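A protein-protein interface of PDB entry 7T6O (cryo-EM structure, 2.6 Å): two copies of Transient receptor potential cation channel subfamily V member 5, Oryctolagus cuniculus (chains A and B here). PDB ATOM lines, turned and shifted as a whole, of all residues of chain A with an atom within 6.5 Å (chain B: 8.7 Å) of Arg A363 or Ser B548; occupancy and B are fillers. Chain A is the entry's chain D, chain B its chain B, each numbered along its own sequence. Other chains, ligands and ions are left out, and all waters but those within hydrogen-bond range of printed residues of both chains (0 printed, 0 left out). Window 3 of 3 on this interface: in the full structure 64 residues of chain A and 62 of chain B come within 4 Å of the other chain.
The backbone NH (N) of Asp B516 lies within hydrogen-bond range of the backbone carbonyl oxygen (O) of Ile A365, at 2.7 Å.
O of Tyr B547 sits at hydrogen-bond distance from NH1 of Arg A363, at 2.7 Å.
The guanidinium group of Arg A363 sits at hydrogen-bond distance from the backbone carbonyl oxygen of Val B549, 2.8 Å away.
The guanidinium group of Arg A363 lies within salt-bridge range of the side-chain carboxylate of Asp B550, at 2.9 Å.
OG1 of Thr A366 sits at hydrogen-bond distance from OE1 of Glu B515 (3.1 Å).
OD1 of Asn B519 lies close to OD2 of Asp B516 (3.0 Å).
OD1 of Asn B546 sits at hydrogen-bond distance from OG of Ser B548 (2.7 Å).
O of Asn B519 lies within hydrogen-bond range of ND2 of Asn B546.
OD1 of Asp A364 is in hydrogen-bond range of N of Thr A366.
Among the printed residues, merely in contact across the chains: Asp A361 with Asp B550, Arg A363 with Ser B548, Ile A365 with Glu B515, Ile A365 with Asn B519, Ile A365 with Val B549 and Ile A365 with Asp B550.
Arg A363 touches just these residues of chain B: Tyr B547, Ser B548, Val B549 and Asp B550.
No residue of chain B comes within 4 Å of Pro A362.
Printed residues of chain B within 4 Å of Ile A365: Glu B515 (3.4 Å), Asp B516 (2.7 Å), Asn B519 (3.3 Å), Val B549 (3.7 Å) and Asp B550 (3.8 Å).
Of the printed residues of chain A, Asp B550 touches Asp A361 (3.8 Å), Arg A363 (2.8 Å) and Ile A365 (3.8 Å).
Of the printed residues of chain A, Asn B519 touches Ile A365 (3.3 Å).
Thr A360 touches none of the printed residues of chain B.
Leu B551 touches none of the printed residues of chain A.
The nearest residue of chain A that does not touch Ser B548 is Pro A362 (4.6 Å).
The nearest printed residue of chain B that does not touch Asp A361 is Val B549 (7.4 Å).
Of the 10 printed residues of chain A, 4 touch a printed residue of chain B.
Printed residues of chain A that touch a printed residue of chain B: Asp A361, Arg A363, Ile A365 and Thr A366.
Hydrophobic or aromatic side chains of chain A that line the printed part of chain B: Ile A365.
Printed residues of chain B that touch a printed residue of chain A: Glu B515, Asp B516, Asn B519, Tyr B547, Ser B548, Val B549 and Asp B550.
Among the printed residues, 11 pairs touch across the chains.
No position is printed for both chains.
Of the 11 pairs that touch across the chains among the printed residues, none has its exchanged pair printed and touching as well.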
ATOM      1  N   THR A 360      -6.134   7.067 -27.065  1.00  0.00           N
ATOM      2  CA  THR A 360      -5.331   6.034 -27.704  1.00  0.00           C
ATOM      3  C   THR A 360      -5.304   4.736 -26.911  1.00  0.00           C
ATOM      4  O   THR A 360      -5.240   3.657 -27.509  1.00  0.00           O
ATOM      5  CB  THR A 360      -3.895   6.526 -27.912  1.00  0.00           C
ATOM      6  OG1 THR A 360      -3.314   6.858 -26.645  1.00  0.00           O
ATOM      7  CG2 THR A 360      -3.882   7.755 -28.808  1.00  0.00           C
ATOM      8  N   ASP A 361      -5.353   4.823 -25.589  1.00  0.00           N
ATOM      9  CA  ASP A 361      -5.402   3.632 -24.754  1.00  0.00           C
ATOM     10  C   ASP A 361      -6.806   3.034 -24.794  1.00  0.00           C
ATOM     11  O   ASP A 361      -7.783   3.752 -24.551  1.00  0.00           O
ATOM     12  CB  ASP A 361      -5.016   3.992 -23.320  1.00  0.00           C
ATOM     13  CG  ASP A 361      -4.558   2.792 -22.512  1.00  0.00           C
ATOM     14  OD1 ASP A 361      -4.252   1.743 -23.112  1.00  0.00           O
ATOM     15  OD2 ASP A 361      -4.502   2.904 -21.270  1.00  0.00           O
ATOM     16  N   PRO A 362      -6.952   1.746 -25.123  1.00  0.00           N
ATOM     17  CA  PRO A 362      -8.275   1.104 -25.008  1.00  0.00           C
ATOM     18  C   PRO A 362      -8.787   0.995 -23.580  1.00  0.00           C
ATOM     19  O   PRO A 362      -9.999   0.845 -23.383  1.00  0.00           O
ATOM     20  CB  PRO A 362      -8.049  -0.282 -25.628  1.00  0.00           C
ATOM     21  CG  PRO A 362      -6.571  -0.493 -25.569  1.00  0.00           C
ATOM     22  CD  PRO A 362      -5.970   0.859 -25.765  1.00  0.00           C
ATOM     23  N   ARG A 363      -7.907   1.058 -22.579  1.00  0.00           N
ATOM     24  CA  ARG A 363      -8.323   1.040 -21.184  1.00  0.00           C
ATOM     25  C   ARG A 363      -8.813   2.396 -20.693  1.00  0.00           C
ATOM     26  O   ARG A 363      -9.416   2.463 -19.618  1.00  0.00           O
ATOM     27  CB  ARG A 363      -7.168   0.567 -20.301  1.00  0.00           C
ATOM     28  CG  ARG A 363      -6.757  -0.871 -20.532  1.00  0.00           C
ATOM     29  CD  ARG A 363      -5.733  -1.322 -19.508  1.00  0.00           C
ATOM     30  NE  ARG A 363      -6.270  -1.313 -18.152  1.00  0.00           N
ATOM     31  CZ  ARG A 363      -6.779  -2.372 -17.541  1.00  0.00           C
ATOM     32  NH1 ARG A 363      -6.853  -3.549 -18.142  1.00  0.00           N
ATOM     33  NH2 ARG A 363      -7.230  -2.249 -16.296  1.00  0.00           N
ATOM     34  N   ASP A 364      -8.570   3.466 -21.447  1.00  0.00           N
ATOM     35  CA  ASP A 364      -8.998   4.801 -21.052  1.00  0.00           C
ATOM     36  C   ASP A 364     -10.474   4.978 -21.386  1.00  0.00           C
ATOM     37  O   ASP A 364     -10.884   4.791 -22.536  1.00  0.00           O
ATOM     38  CB  ASP A 364      -8.150   5.858 -21.758  1.00  0.00           C
ATOM     39  CG  ASP A 364      -8.398   7.259 -21.230  1.00  0.00           C
ATOM     40  OD1 ASP A 364      -8.942   7.400 -20.116  1.00  0.00           O
ATOM     41  OD2 ASP A 364      -8.047   8.228 -21.936  1.00  0.00           O
ATOM     42  N   ILE A 365     -11.273   5.328 -20.379  1.00  0.00           N
ATOM     43  CA  ILE A 365     -12.706   5.538 -20.544  1.00  0.00           C
ATOM     44  C   ILE A 365     -13.133   6.954 -20.208  1.00  0.00           C
ATOM     45  O   ILE A 365     -14.336   7.229 -20.168  1.00  0.00           O
ATOM     46  CB  ILE A 365     -13.523   4.529 -19.713  1.00  0.00           C
ATOM     47  CG1 ILE A 365     -13.218   4.688 -18.224  1.00  0.00           C
ATOM     48  CG2 ILE A 365     -13.244   3.126 -20.177  1.00  0.00           C
ATOM     49  CD1 ILE A 365     -14.168   3.938 -17.321  1.00  0.00           C
ATOM     50  N   THR A 366     -12.190   7.858 -19.958  1.00  0.00           N
ATOM     51  CA  THR A 366     -12.526   9.241 -19.653  1.00  0.00           C
ATOM     52  C   THR A 366     -13.025   9.934 -20.916  1.00  0.00           C
ATOM     53  O   THR A 366     -12.316   9.992 -21.924  1.00  0.00           O
ATOM     54  CB  THR A 366     -11.309   9.964 -19.078  1.00  0.00           C
ATOM     55  OG1 THR A 366     -11.046   9.477 -17.759  1.00  0.00           O
ATOM     56  CG2 THR A 366     -11.556  11.457 -19.005  1.00  0.00           C
ATOM     57  N   ASN A 518      -6.532 -11.125 -19.579  1.00  0.00           N
ATOM     58  CA  ASN A 518      -7.805 -10.870 -20.245  1.00  0.00           C
ATOM     59  C   ASN A 518      -8.870 -11.893 -19.874  1.00  0.00           C
ATOM     60  O   ASN A 518     -10.063 -11.608 -20.020  1.00  0.00           O
ATOM     61  CB  ASN A 518      -7.610 -10.847 -21.760  1.00  0.00           C
ATOM     62  CG  ASN A 518      -6.521  -9.886 -22.192  1.00  0.00           C
ATOM     63  OD1 ASN A 518      -6.312  -8.846 -21.567  1.00  0.00           O
ATOM     64  ND2 ASN A 518      -5.818 -10.230 -23.263  1.00  0.00           N
ATOM     65  N   SER A 524      -4.235  -8.981 -11.858  1.00  0.00           N
ATOM     66  CA  SER A 524      -3.333  -8.733 -12.981  1.00  0.00           C
ATOM     67  C   SER A 524      -2.059  -8.026 -12.535  1.00  0.00           C
ATOM     68  O   SER A 524      -0.958  -8.396 -12.958  1.00  0.00           O
ATOM     69  CB  SER A 524      -4.054  -7.924 -14.058  1.00  0.00           C
ATOM     70  OG  SER A 524      -4.592  -6.728 -13.522  1.00  0.00           O
ATOM     71  N   THR A 528      -4.172  -4.006  -7.899  1.00  0.00           N
ATOM     72  CA  THR A 528      -5.453  -4.600  -8.269  1.00  0.00           C
ATOM     73  C   THR A 528      -5.701  -5.891  -7.501  1.00  0.00           C
ATOM     74  O   THR A 528      -6.827  -6.156  -7.069  1.00  0.00           O
ATOM     75  CB  THR A 528      -5.500  -4.855  -9.776  1.00  0.00           C
ATOM     76  OG1 THR A 528      -5.171  -3.649 -10.474  1.00  0.00           O
ATOM     77  CG2 THR A 528      -6.882  -5.317 -10.219  1.00  0.00           C
ATOM     78  N   GLU B 515     -16.467   9.718 -16.941  1.00  0.00           N
ATOM     79  CA  GLU B 515     -16.123   8.445 -17.555  1.00  0.00           C
ATOM     80  C   GLU B 515     -17.246   7.968 -18.467  1.00  0.00           C
ATOM     81  O   GLU B 515     -18.367   8.481 -18.434  1.00  0.00           O
ATOM     82  CB  GLU B 515     -15.826   7.387 -16.487  1.00  0.00           C
ATOM     83  CG  GLU B 515     -15.011   7.900 -15.312  1.00  0.00           C
ATOM     84  CD  GLU B 515     -13.597   8.285 -15.697  1.00  0.00           C
ATOM     85  OE1 GLU B 515     -12.933   7.496 -16.398  1.00  0.00           O
ATOM     86  OE2 GLU B 515     -13.147   9.379 -15.298  1.00  0.00           O
ATOM     87  N   ASP B 516     -16.921   6.973 -19.284  1.00  0.00           N
ATOM     88  CA  ASP B 516     -17.882   6.403 -20.220  1.00  0.00           C
ATOM     89  C   ASP B 516     -18.866   5.514 -19.468  1.00  0.00           C
ATOM     90  O   ASP B 516     -18.438   4.572 -18.790  1.00  0.00           O
ATOM     91  CB  ASP B 516     -17.150   5.599 -21.288  1.00  0.00           C
ATOM     92  CG  ASP B 516     -18.021   5.270 -22.482  1.00  0.00           C
ATOM     93  OD1 ASP B 516     -19.029   5.969 -22.708  1.00  0.00           O
ATOM     94  OD2 ASP B 516     -17.694   4.306 -23.203  1.00  0.00           O
ATOM     95  N   ASN B 519     -19.023   1.380 -20.013  1.00  0.00           N
ATOM     96  CA  ASN B 519     -18.084   0.465 -19.377  1.00  0.00           C
ATOM     97  C   ASN B 519     -18.460   0.184 -17.928  1.00  0.00           C
ATOM     98  O   ASN B 519     -18.346  -0.955 -17.463  1.00  0.00           O
ATOM     99  CB  ASN B 519     -16.668   1.033 -19.472  1.00  0.00           C
ATOM    100  CG  ASN B 519     -16.235   1.266 -20.905  1.00  0.00           C
ATOM    101  OD1 ASN B 519     -16.231   2.395 -21.388  1.00  0.00           O
ATOM    102  ND2 ASN B 519     -15.869   0.192 -21.594  1.00  0.00           N
ATOM    103  N   ALA B 545     -16.886  -3.531 -11.118  1.00  0.00           N
ATOM    104  CA  ALA B 545     -15.528  -3.827 -11.536  1.00  0.00           C
ATOM    105  C   ALA B 545     -15.495  -4.002 -13.045  1.00  0.00           C
ATOM    106  O   ALA B 545     -16.437  -4.526 -13.646  1.00  0.00           O
ATOM    107  CB  ALA B 545     -14.984  -5.083 -10.847  1.00  0.00           C
ATOM    108  N   ASN B 546     -14.399  -3.551 -13.648  1.00  0.00           N
ATOM    109  CA  ASN B 546     -14.163  -3.738 -15.077  1.00  0.00           C
ATOM    110  C   ASN B 546     -12.649  -3.772 -15.253  1.00  0.00           C
ATOM    111  O   ASN B 546     -12.000  -2.722 -15.270  1.00  0.00           O
ATOM    112  CB  ASN B 546     -14.809  -2.631 -15.898  1.00  0.00           C
ATOM    113  CG  ASN B 546     -14.973  -3.000 -17.362  1.00  0.00           C
ATOM    114  OD1 ASN B 546     -14.341  -3.928 -17.859  1.00  0.00           O
ATOM    115  ND2 ASN B 546     -15.828  -2.266 -18.060  1.00  0.00           N
ATOM    116  N   TYR B 547     -12.098  -4.977 -15.372  1.00  0.00           N
ATOM    117  CA  TYR B 547     -10.655  -5.159 -15.409  1.00  0.00           C
ATOM    118  C   TYR B 547     -10.064  -4.958 -16.795  1.00  0.00           C
ATOM    119  O   TYR B 547      -8.837  -4.930 -16.929  1.00  0.00           O
ATOM    120  CB  TYR B 547     -10.296  -6.552 -14.882  1.00  0.00           C
ATOM    121  CG  TYR B 547     -10.839  -6.803 -13.496  1.00  0.00           C
ATOM    122  CD1 TYR B 547     -10.310  -6.141 -12.395  1.00  0.00           C
ATOM    123  CD2 TYR B 547     -11.893  -7.682 -13.290  1.00  0.00           C
ATOM    124  CE1 TYR B 547     -10.806  -6.358 -11.127  1.00  0.00           C
ATOM    125  CE2 TYR B 547     -12.398  -7.903 -12.026  1.00  0.00           C
ATOM    126  CZ  TYR B 547     -11.849  -7.240 -10.949  1.00  0.00           C
ATOM    127  OH  TYR B 547     -12.346  -7.457  -9.686  1.00  0.00           O
ATOM    128  N   SER B 548     -10.897  -4.812 -17.818  1.00  0.00           N
ATOM    129  CA  SER B 548     -10.428  -4.497 -19.158  1.00  0.00           C
ATOM    130  C   SER B 548     -10.185  -3.008 -19.359  1.00  0.00           C
ATOM    131  O   SER B 548      -9.589  -2.622 -20.369  1.00  0.00           O
ATOM    132  CB  SER B 548     -11.432  -5.002 -20.197  1.00  0.00           C
ATOM    133  OG  SER B 548     -12.723  -4.472 -19.955  1.00  0.00           O
ATOM    134  N   VAL B 549     -10.642  -2.165 -18.429  1.00  0.00           N
ATOM    135  CA  VAL B 549     -10.481  -0.721 -18.513  1.00  0.00           C
ATOM    136  C   VAL B 549      -9.833  -0.228 -17.226  1.00  0.00           C
ATOM    137  O   VAL B 549      -9.710  -0.960 -16.242  1.00  0.00           O
ATOM    138  CB  VAL B 549     -11.820   0.018 -18.748  1.00  0.00           C
ATOM    139  CG1 VAL B 549     -12.572  -0.551 -19.947  1.00  0.00           C
ATOM    140  CG2 VAL B 549     -12.684  -0.018 -17.500  1.00  0.00           C
ATOM    141  N   ASP B 550      -9.414   1.035 -17.247  1.00  0.00           N
ATOM    142  CA  ASP B 550      -8.850   1.683 -16.069  1.00  0.00           C
ATOM    143  C   ASP B 550      -9.929   2.513 -15.385  1.00  0.00           C
ATOM    144  O   ASP B 550     -10.467   3.454 -15.979  1.00  0.00           O
ATOM    145  CB  ASP B 550      -7.658   2.563 -16.444  1.00  0.00           C
ATOM    146  CG  ASP B 550      -6.424   1.758 -16.793  1.00  0.00           C
ATOM    147  OD1 ASP B 550      -6.146   0.757 -16.098  1.00  0.00           O
ATOM    148  OD2 ASP B 550      -5.722   2.132 -17.756  1.00  0.00           O
ATOM    149  N   LEU B 551     -10.239   2.166 -14.150  1.00  0.00           N
ATOM    150  CA  LEU B 551     -11.172   2.889 -13.306  1.00  0.00           C
ATOM    151  C   LEU B 551     -10.446   3.995 -12.552  1.00  0.00           C
ATOM    152  O   LEU B 551      -9.222   3.948 -12.400  1.00  0.00           O
ATOM    153  CB  LEU B 551     -11.847   1.922 -12.322  1.00  0.00           C
ATOM    154  CG  LEU B 551     -12.677   0.802 -12.958  1.00  0.00           C
ATOM    155  CD1 LEU B 551     -13.423   0.009 -11.899  1.00  0.00           C
ATOM    156  CD2 LEU B 551     -13.642   1.353 -13.995  1.00  0.00           C
ATOM    157  N   PRO B 552     -11.158   5.039 -12.112  1.00  0.00           N
ATOM    158  CA  PRO B 552     -10.513   6.068 -11.284  1.00  0.00           C
ATOM    159  C   PRO B 552     -10.051   5.521  -9.941  1.00  0.00           C
ATOM    160  O   PRO B 552     -10.672   4.626  -9.364  1.00  0.00           O
ATOM    161  CB  PRO B 552     -11.612   7.122 -11.109  1.00  0.00           C
ATOM    162  CG  PRO B 552     -12.507   6.934 -12.268  1.00  0.00           C
ATOM    163  CD  PRO B 552     -12.489   5.472 -12.580  1.00  0.00           C
